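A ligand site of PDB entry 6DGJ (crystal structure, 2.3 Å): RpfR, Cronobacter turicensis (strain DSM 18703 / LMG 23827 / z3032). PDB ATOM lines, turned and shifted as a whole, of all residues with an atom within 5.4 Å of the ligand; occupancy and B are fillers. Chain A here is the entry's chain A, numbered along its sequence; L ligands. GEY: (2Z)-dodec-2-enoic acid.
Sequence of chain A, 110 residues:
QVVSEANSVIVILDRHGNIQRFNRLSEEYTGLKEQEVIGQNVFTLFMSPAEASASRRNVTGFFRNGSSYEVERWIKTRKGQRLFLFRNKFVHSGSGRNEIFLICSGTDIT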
ATOM      1  N   VAL A  11      -9.964 -26.194 -16.208  1.00  0.00           N
ATOM      2  CA  VAL A  11      -9.974 -24.838 -16.733  1.00  0.00           C
ATOM      3  C   VAL A  11      -9.184 -23.957 -15.783  1.00  0.00           C
ATOM      4  O   VAL A  11      -9.391 -24.003 -14.563  1.00  0.00           O
ATOM      5  CB  VAL A  11     -11.411 -24.304 -16.912  1.00  0.00           C
ATOM      6  CG1 VAL A  11     -11.405 -22.924 -17.528  1.00  0.00           C
ATOM      7  CG2 VAL A  11     -12.237 -25.268 -17.761  1.00  0.00           C
ATOM      8  N   LEU A  13      -8.263 -20.054 -14.787  1.00  0.00           N
ATOM      9  CA  LEU A  13      -8.886 -18.739 -14.869  1.00  0.00           C
ATOM     10  C   LEU A  13      -7.997 -17.697 -14.210  1.00  0.00           C
ATOM     11  O   LEU A  13      -7.111 -18.009 -13.411  1.00  0.00           O
ATOM     12  CB  LEU A  13     -10.266 -18.735 -14.197  1.00  0.00           C
ATOM     13  CG  LEU A  13     -11.175 -19.930 -14.493  1.00  0.00           C
ATOM     14  CD1 LEU A  13     -12.367 -19.923 -13.550  1.00  0.00           C
ATOM     15  CD2 LEU A  13     -11.642 -19.908 -15.938  1.00  0.00           C
ATOM     16  N   PHE A  22      -7.826 -24.808 -21.278  1.00  0.00           N
ATOM     17  CA  PHE A  22      -9.125 -25.438 -21.532  1.00  0.00           C
ATOM     18  C   PHE A  22      -8.837 -26.844 -22.061  1.00  0.00           C
ATOM     19  O   PHE A  22      -8.671 -27.045 -23.269  1.00  0.00           O
ATOM     20  CB  PHE A  22      -9.921 -24.603 -22.522  1.00  0.00           C
ATOM     21  CG  PHE A  22     -11.387 -24.923 -22.561  1.00  0.00           C
ATOM     22  CD1 PHE A  22     -12.211 -24.621 -21.488  1.00  0.00           C
ATOM     23  CD2 PHE A  22     -11.960 -25.489 -23.683  1.00  0.00           C
ATOM     24  CE1 PHE A  22     -13.556 -24.908 -21.522  1.00  0.00           C
ATOM     25  CE2 PHE A  22     -13.314 -25.781 -23.735  1.00  0.00           C
ATOM     26  CZ  PHE A  22     -14.117 -25.481 -22.648  1.00  0.00           C
ATOM     27  N   SER A  26     -12.924 -30.655 -21.603  1.00  0.00           N
ATOM     28  CA  SER A  26     -13.776 -29.472 -21.643  1.00  0.00           C
ATOM     29  C   SER A  26     -14.207 -29.140 -23.067  1.00  0.00           C
ATOM     30  O   SER A  26     -15.314 -28.638 -23.267  1.00  0.00           O
ATOM     31  CB  SER A  26     -13.038 -28.283 -21.023  1.00  0.00           C
ATOM     32  OG  SER A  26     -12.586 -28.569 -19.708  1.00  0.00           O
ATOM     33  N   TYR A  29     -17.091 -31.497 -24.017  1.00  0.00           N
ATOM     34  CA  TYR A  29     -18.354 -31.155 -23.378  1.00  0.00           C
ATOM     35  C   TYR A  29     -19.029 -29.956 -24.038  1.00  0.00           C
ATOM     36  O   TYR A  29     -20.254 -29.860 -24.047  1.00  0.00           O
ATOM     37  CB  TYR A  29     -18.146 -30.863 -21.889  1.00  0.00           C
ATOM     38  CG  TYR A  29     -18.380 -32.057 -20.984  1.00  0.00           C
ATOM     39  CD1 TYR A  29     -19.667 -32.447 -20.634  1.00  0.00           C
ATOM     40  CD2 TYR A  29     -17.309 -32.781 -20.455  1.00  0.00           C
ATOM     41  CE1 TYR A  29     -19.895 -33.525 -19.800  1.00  0.00           C
ATOM     42  CE2 TYR A  29     -17.525 -33.866 -19.625  1.00  0.00           C
ATOM     43  CZ  TYR A  29     -18.813 -34.225 -19.302  1.00  0.00           C
ATOM     44  OH  TYR A  29     -19.025 -35.308 -18.463  1.00  0.00           O
ATOM     45  N   THR A  30     -18.234 -29.049 -24.615  1.00  0.00           N
ATOM     46  CA  THR A  30     -18.751 -27.775 -25.106  1.00  0.00           C
ATOM     47  C   THR A  30     -18.749 -27.644 -26.618  1.00  0.00           C
ATOM     48  O   THR A  30     -19.510 -26.831 -27.150  1.00  0.00           O
ATOM     49  CB  THR A  30     -17.923 -26.610 -24.532  1.00  0.00           C
ATOM     50  OG1 THR A  30     -16.558 -26.736 -24.949  1.00  0.00           O
ATOM     51  CG2 THR A  30     -17.996 -26.608 -23.025  1.00  0.00           C
ATOM     52  N   VAL A  42     -15.494 -17.143 -18.573  1.00  0.00           N
ATOM     53  CA  VAL A  42     -16.094 -18.452 -18.350  1.00  0.00           C
ATOM     54  C   VAL A  42     -17.522 -18.322 -17.826  1.00  0.00           C
ATOM     55  O   VAL A  42     -18.388 -19.141 -18.139  1.00  0.00           O
ATOM     56  CB  VAL A  42     -15.211 -19.290 -17.399  1.00  0.00           C
ATOM     57  CG1 VAL A  42     -15.286 -18.761 -15.963  1.00  0.00           C
ATOM     58  CG2 VAL A  42     -15.614 -20.762 -17.444  1.00  0.00           C
ATOM     59  N   PHE A  46     -20.440 -20.306 -20.043  1.00  0.00           N
ATOM     60  CA  PHE A  46     -20.769 -21.682 -19.661  1.00  0.00           C
ATOM     61  C   PHE A  46     -21.690 -21.802 -18.459  1.00  0.00           C
ATOM     62  O   PHE A  46     -21.861 -22.904 -17.936  1.00  0.00           O
ATOM     63  CB  PHE A  46     -19.476 -22.454 -19.368  1.00  0.00           C
ATOM     64  CG  PHE A  46     -18.577 -22.607 -20.562  1.00  0.00           C
ATOM     65  CD1 PHE A  46     -19.073 -23.095 -21.757  1.00  0.00           C
ATOM     66  CD2 PHE A  46     -17.232 -22.265 -20.494  1.00  0.00           C
ATOM     67  CE1 PHE A  46     -18.257 -23.242 -22.858  1.00  0.00           C
ATOM     68  CE2 PHE A  46     -16.412 -22.410 -21.585  1.00  0.00           C
ATOM     69  CZ  PHE A  46     -16.925 -22.904 -22.772  1.00  0.00           C
ATOM     70  N   MET A  47     -22.312 -20.709 -18.005  1.00  0.00           N
ATOM     71  CA  MET A  47     -23.243 -20.825 -16.888  1.00  0.00           C
ATOM     72  C   MET A  47     -24.328 -19.760 -17.000  1.00  0.00           C
ATOM     73  O   MET A  47     -24.135 -18.708 -17.623  1.00  0.00           O
ATOM     74  CB  MET A  47     -22.520 -20.738 -15.537  1.00  0.00           C
ATOM     75  CG  MET A  47     -21.462 -19.657 -15.431  1.00  0.00           C
ATOM     76  SD  MET A  47     -20.509 -19.778 -13.886  1.00  0.00           S
ATOM     77  CE  MET A  47     -19.531 -21.259 -14.178  1.00  0.00           C
ATOM     78  N   ALA A  54     -23.324 -16.170  -8.562  1.00  0.00           N
ATOM     79  CA  ALA A  54     -22.709 -16.754  -7.374  1.00  0.00           C
ATOM     80  C   ALA A  54     -21.260 -17.143  -7.642  1.00  0.00           C
ATOM     81  O   ALA A  54     -20.394 -16.971  -6.775  1.00  0.00           O
ATOM     82  CB  ALA A  54     -23.506 -17.975  -6.911  1.00  0.00           C
ATOM     83  N   SER A  55     -20.973 -17.672  -8.827  1.00  0.00           N
ATOM     84  CA  SER A  55     -19.611 -18.082  -9.141  1.00  0.00           C
ATOM     85  C   SER A  55     -18.674 -16.883  -9.238  1.00  0.00           C
ATOM     86  O   SER A  55     -17.560 -16.912  -8.701  1.00  0.00           O
ATOM     87  CB  SER A  55     -19.596 -18.872 -10.452  1.00  0.00           C
ATOM     88  OG  SER A  55     -18.290 -19.324 -10.765  1.00  0.00           O
ATOM     89  N   ASN A  58     -17.531 -15.795  -5.968  1.00  0.00           N
ATOM     90  CA  ASN A  58     -16.571 -16.726  -5.379  1.00  0.00           C
ATOM     91  C   ASN A  58     -15.167 -16.450  -5.894  1.00  0.00           C
ATOM     92  O   ASN A  58     -14.225 -16.307  -5.101  1.00  0.00           O
ATOM     93  CB  ASN A  58     -16.979 -18.168  -5.686  1.00  0.00           C
ATOM     94  CG  ASN A  58     -18.288 -18.564  -5.022  1.00  0.00           C
ATOM     95  OD1 ASN A  58     -18.897 -17.764  -4.303  1.00  0.00           O
ATOM     96  ND2 ASN A  58     -18.725 -19.791  -5.269  1.00  0.00           N
ATOM     97  N   VAL A  59     -15.010 -16.372  -7.210  1.00  0.00           N
ATOM     98  CA  VAL A  59     -13.689 -16.171  -7.796  1.00  0.00           C
ATOM     99  C   VAL A  59     -13.104 -14.841  -7.335  1.00  0.00           C
ATOM    100  O   VAL A  59     -11.916 -14.756  -6.988  1.00  0.00           O
ATOM    101  CB  VAL A  59     -13.773 -16.251  -9.338  1.00  0.00           C
ATOM    102  CG1 VAL A  59     -12.403 -16.013  -9.965  1.00  0.00           C
ATOM    103  CG2 VAL A  59     -14.322 -17.599  -9.767  1.00  0.00           C
ATOM    104  N   TYR A  69     -10.897 -24.791  -1.949  1.00  0.00           N
ATOM    105  CA  TYR A  69     -12.275 -25.151  -1.619  1.00  0.00           C
ATOM    106  C   TYR A  69     -12.869 -25.938  -2.765  1.00  0.00           C
ATOM    107  O   TYR A  69     -12.311 -25.986  -3.869  1.00  0.00           O
ATOM    108  CB  TYR A  69     -13.110 -23.896  -1.335  1.00  0.00           C
ATOM    109  CG  TYR A  69     -13.369 -23.061  -2.580  1.00  0.00           C
ATOM    110  CD1 TYR A  69     -12.406 -22.186  -3.060  1.00  0.00           C
ATOM    111  CD2 TYR A  69     -14.564 -23.162  -3.267  1.00  0.00           C
ATOM    112  CE1 TYR A  69     -12.636 -21.431  -4.190  1.00  0.00           C
ATOM    113  CE2 TYR A  69     -14.807 -22.412  -4.402  1.00  0.00           C
ATOM    114  CZ  TYR A  69     -13.841 -21.545  -4.859  1.00  0.00           C
ATOM    115  OH  TYR A  69     -14.077 -20.803  -5.984  1.00  0.00           O
ATOM    116  N   VAL A  71     -16.647 -26.727  -4.920  1.00  0.00           N
ATOM    117  CA  VAL A  71     -17.900 -26.082  -5.284  1.00  0.00           C
ATOM    118  C   VAL A  71     -18.622 -26.952  -6.299  1.00  0.00           C
ATOM    119  O   VAL A  71     -17.997 -27.633  -7.117  1.00  0.00           O
ATOM    120  CB  VAL A  71     -17.666 -24.662  -5.843  1.00  0.00           C
ATOM    121  CG1 VAL A  71     -16.819 -24.709  -7.112  1.00  0.00           C
ATOM    122  CG2 VAL A  71     -18.990 -23.953  -6.099  1.00  0.00           C
ATOM    123  N   ARG A  73     -21.185 -26.582  -9.374  1.00  0.00           N
ATOM    124  CA  ARG A  73     -21.639 -25.548 -10.302  1.00  0.00           C
ATOM    125  C   ARG A  73     -22.345 -26.206 -11.468  1.00  0.00           C
ATOM    126  O   ARG A  73     -21.762 -27.067 -12.141  1.00  0.00           O
ATOM    127  CB  ARG A  73     -20.457 -24.702 -10.786  1.00  0.00           C
ATOM    128  CG  ARG A  73     -20.860 -23.453 -11.569  1.00  0.00           C
ATOM    129  CD  ARG A  73     -21.579 -22.452 -10.684  1.00  0.00           C
ATOM    130  NE  ARG A  73     -20.742 -21.974  -9.586  1.00  0.00           N
ATOM    131  CZ  ARG A  73     -21.217 -21.450  -8.470  1.00  0.00           C
ATOM    132  NH1 ARG A  73     -22.521 -21.321  -8.272  1.00  0.00           N
ATOM    133  NH2 ARG A  73     -20.379 -21.041  -7.526  1.00  0.00           N
ATOM    134  N   ILE A  75     -23.073 -26.444 -14.976  1.00  0.00           N
ATOM    135  CA  ILE A  75     -22.367 -25.975 -16.162  1.00  0.00           C
ATOM    136  C   ILE A  75     -23.240 -26.217 -17.380  1.00  0.00           C
ATOM    137  O   ILE A  75     -24.049 -27.143 -17.429  1.00  0.00           O
ATOM    138  CB  ILE A  75     -20.990 -26.682 -16.299  1.00  0.00           C
ATOM    139  CG1 ILE A  75     -20.118 -26.398 -15.078  1.00  0.00           C
ATOM    140  CG2 ILE A  75     -20.280 -26.236 -17.583  1.00  0.00           C
ATOM    141  CD1 ILE A  75     -19.830 -24.926 -14.823  1.00  0.00           C
ATOM    142  N   LYS A  76     -23.043 -25.369 -18.377  1.00  0.00           N
ATOM    143  CA  LYS A  76     -23.888 -25.302 -19.570  1.00  0.00           C
ATOM    144  C   LYS A  76     -23.126 -25.938 -20.727  1.00  0.00           C
ATOM    145  O   LYS A  76     -22.177 -25.345 -21.255  1.00  0.00           O
ATOM    146  CB  LYS A  76     -24.239 -23.844 -19.826  1.00  0.00           C
ATOM    147  CG  LYS A  76     -24.933 -23.493 -21.111  1.00  0.00           C
ATOM    148  CD  LYS A  76     -25.166 -21.993 -21.095  1.00  0.00           C
ATOM    149  CE  LYS A  76     -25.770 -21.441 -22.372  1.00  0.00           C
ATOM    150  NZ  LYS A  76     -25.831 -19.962 -22.284  1.00  0.00           N
ATOM    151  N   THR A  77     -23.522 -27.144 -21.108  1.00  0.00           N
ATOM    152  CA  THR A  77     -22.775 -27.968 -22.053  1.00  0.00           C
ATOM    153  C   THR A  77     -23.577 -28.197 -23.329  1.00  0.00           C
ATOM    154  O   THR A  77     -24.680 -27.693 -23.498  1.00  0.00           O
ATOM    155  CB  THR A  77     -22.407 -29.320 -21.424  1.00  0.00           C
ATOM    156  OG1 THR A  77     -23.556 -30.173 -21.399  1.00  0.00           O
ATOM    157  CG2 THR A  77     -21.887 -29.143 -19.998  1.00  0.00           C
ATOM    158  N   PHE A  86     -16.117 -28.835  -8.724  1.00  0.00           N
ATOM    159  CA  PHE A  86     -14.848 -28.206  -9.047  1.00  0.00           C
ATOM    160  C   PHE A  86     -13.997 -28.077  -7.785  1.00  0.00           C
ATOM    161  O   PHE A  86     -14.464 -27.576  -6.758  1.00  0.00           O
ATOM    162  CB  PHE A  86     -15.054 -26.818  -9.680  1.00  0.00           C
ATOM    163  CG  PHE A  86     -15.405 -26.884 -11.138  1.00  0.00           C
ATOM    164  CD1 PHE A  86     -14.421 -27.092 -12.090  1.00  0.00           C
ATOM    165  CD2 PHE A  86     -16.717 -26.739 -11.553  1.00  0.00           C
ATOM    166  CE1 PHE A  86     -14.736 -27.151 -13.432  1.00  0.00           C
ATOM    167  CE2 PHE A  86     -17.041 -26.801 -12.889  1.00  0.00           C
ATOM    168  CZ  PHE A  86     -16.056 -26.999 -13.834  1.00  0.00           C
ATOM    169  N   ASN A  88     -11.016 -26.077  -6.517  1.00  0.00           N
ATOM    170  CA  ASN A  88     -10.413 -24.816  -6.899  1.00  0.00           C
ATOM    171  C   ASN A  88      -9.279 -24.439  -5.950  1.00  0.00           C
ATOM    172  O   ASN A  88      -9.414 -24.567  -4.735  1.00  0.00           O
ATOM    173  CB  ASN A  88     -11.467 -23.705  -6.923  1.00  0.00           C
ATOM    174  CG  ASN A  88     -12.545 -23.958  -7.956  1.00  0.00           C
ATOM    175  OD1 ASN A  88     -12.316 -24.607  -8.968  1.00  0.00           O
ATOM    176  ND2 ASN A  88     -13.738 -23.437  -7.697  1.00  0.00           N
ATOM    177  N   LEU A 102      -6.085 -19.315 -11.358  1.00  0.00           N
ATOM    178  CA  LEU A 102      -6.896 -20.208 -10.553  1.00  0.00           C
ATOM    179  C   LEU A 102      -7.126 -21.489 -11.341  1.00  0.00           C
ATOM    180  O   LEU A 102      -7.680 -21.454 -12.448  1.00  0.00           O
ATOM    181  CB  LEU A 102      -8.227 -19.551 -10.181  1.00  0.00           C
ATOM    182  CG  LEU A 102      -9.321 -20.458  -9.590  1.00  0.00           C
ATOM    183  CD1 LEU A 102      -8.784 -21.196  -8.379  1.00  0.00           C
ATOM    184  CD2 LEU A 102     -10.545 -19.635  -9.221  1.00  0.00           C
ATOM    185  N   CYS A 104      -9.072 -24.931 -11.886  1.00  0.00           N
ATOM    186  CA  CYS A 104     -10.380 -25.500 -11.601  1.00  0.00           C
ATOM    187  C   CYS A 104     -10.375 -26.951 -12.071  1.00  0.00           C
ATOM    188  O   CYS A 104     -10.304 -27.218 -13.278  1.00  0.00           O
ATOM    189  CB  CYS A 104     -11.479 -24.697 -12.291  1.00  0.00           C
ATOM    190  SG  CYS A 104     -11.541 -22.937 -11.823  1.00  0.00           S
HETATM  191  C1  GEY L   1     -16.797 -20.954  -7.933  1.00  0.00           C
HETATM  192  C2  GEY L   1     -15.476 -20.671  -8.602  1.00  0.00           C
HETATM  193  C3  GEY L   1     -14.975 -21.321  -9.660  1.00  0.00           C
HETATM  194  C4  GEY L   1     -15.686 -22.439 -10.340  1.00  0.00           C
HETATM  195  C5  GEY L   1     -15.026 -22.946 -11.632  1.00  0.00           C
HETATM  196  C6  GEY L   1     -15.988 -23.218 -12.816  1.00  0.00           C
HETATM  197  C8  GEY L   1     -16.323 -23.503 -15.398  1.00  0.00           C
HETATM  198  O2  GEY L   1     -17.794 -20.985  -8.646  1.00  0.00           O
HETATM  199  O1  GEY L   1     -16.761 -21.136  -6.696  1.00  0.00           O
HETATM  200  C7  GEY L   1     -15.351 -23.207 -14.224  1.00  0.00           C
HETATM  201  C9  GEY L   1     -15.759 -24.357 -16.555  1.00  0.00           C
HETATM  202  C10 GEY L   1     -16.823 -25.107 -17.383  1.00  0.00           C
HETATM  203  C11 GEY L   1     -16.414 -25.444 -18.820  1.00  0.00           C
HETATM  204  C12 GEY L   1     -17.523 -26.052 -19.667  1.00  0.00           C
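Val 11 touches the ligand. CE1 of Phe 22 touches C11 of the ligand, 3.97 Å away. Thr 30 touches the ligand. Val 42 touches the ligand (CG2 to C8, 3.5 Å). CD2 of Phe 46 touches C11 of the ligand (3.7 Å). Val 59 touches the ligand (CG2 to C2, 3.5 Å). CG1 of Val 71 touches O1 of the ligand, 3.6 Å away. Ile 75 touches the ligand (CG2 to C12, 3.5 Å). Phe 86 touches the ligand. Asn 88 touches the ligand (ND2 to C3, 3.1 Å). SG of Cys 104 touches C5 of the ligand (3.5 Å). Hydrophobic or aromatic side chains that line the ligand: Val 11, Phe 22, Val 42, Phe 46, Val 59, Tyr 69, Val 71, Ile 75 and Phe 86. 15 residues have an atom within 4 Å of the ligand: Val 11, Phe 22, Thr 30, Val 42, Phe 46, Ser 55, Asn 58, Val 59, Tyr 69, Val 71, Arg 73, Ile 75, Phe 86, Asn 88 and Cys 104. The nearest printed residue that does not touch the ligand is Met 47 (4.1 Å).
OD1 of Asn 88 sits close to SG of Cys 104, 3.4 Å away. The backbone carbonyl oxygen (O) of Ser 26 is in hydrogen-bond range of the side-chain hydroxyl (OG1) of Thr 30 (2.8 Å). O of Val 71 is in hydrogen-bond range of N of Phe 86 (2.7 Å). The backbone carbonyl oxygen (O) of Ala 54 sits close to the side-chain amide oxygen (OD1) of Asn 58 (3.0 Å). The backbone carbonyl oxygen (O) of Phe 46 sits at hydrogen-bond distance from the backbone NH (N) of Lys 76 (2.8 Å). The backbone NH of Cys 104 sits at hydrogen-bond distance from the backbone carbonyl oxygen of Val 11 (2.9 Å). N of Asn 88 is in hydrogen-bond range of O of Tyr 69, 2.9 Å away. The side-chain amide nitrogen (ND2) of Asn 58 lies close to the guanidinium group (NH2) of Arg 73.
OH of Tyr 69 is in hydrogen-bond range of O1 of the ligand (2.8 Å). An oxygen (O2) of the ligand is in salt-bridge range of the guanidinium group (NH2) of Arg 73 (2.8 Å). OG of Ser 55 sits at hydrogen-bond distance from O2 of the ligand, 2.7 Å away. The side-chain amide nitrogen of Asn 58 lies within hydrogen-bond range of an oxygen (O1) of the ligand.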
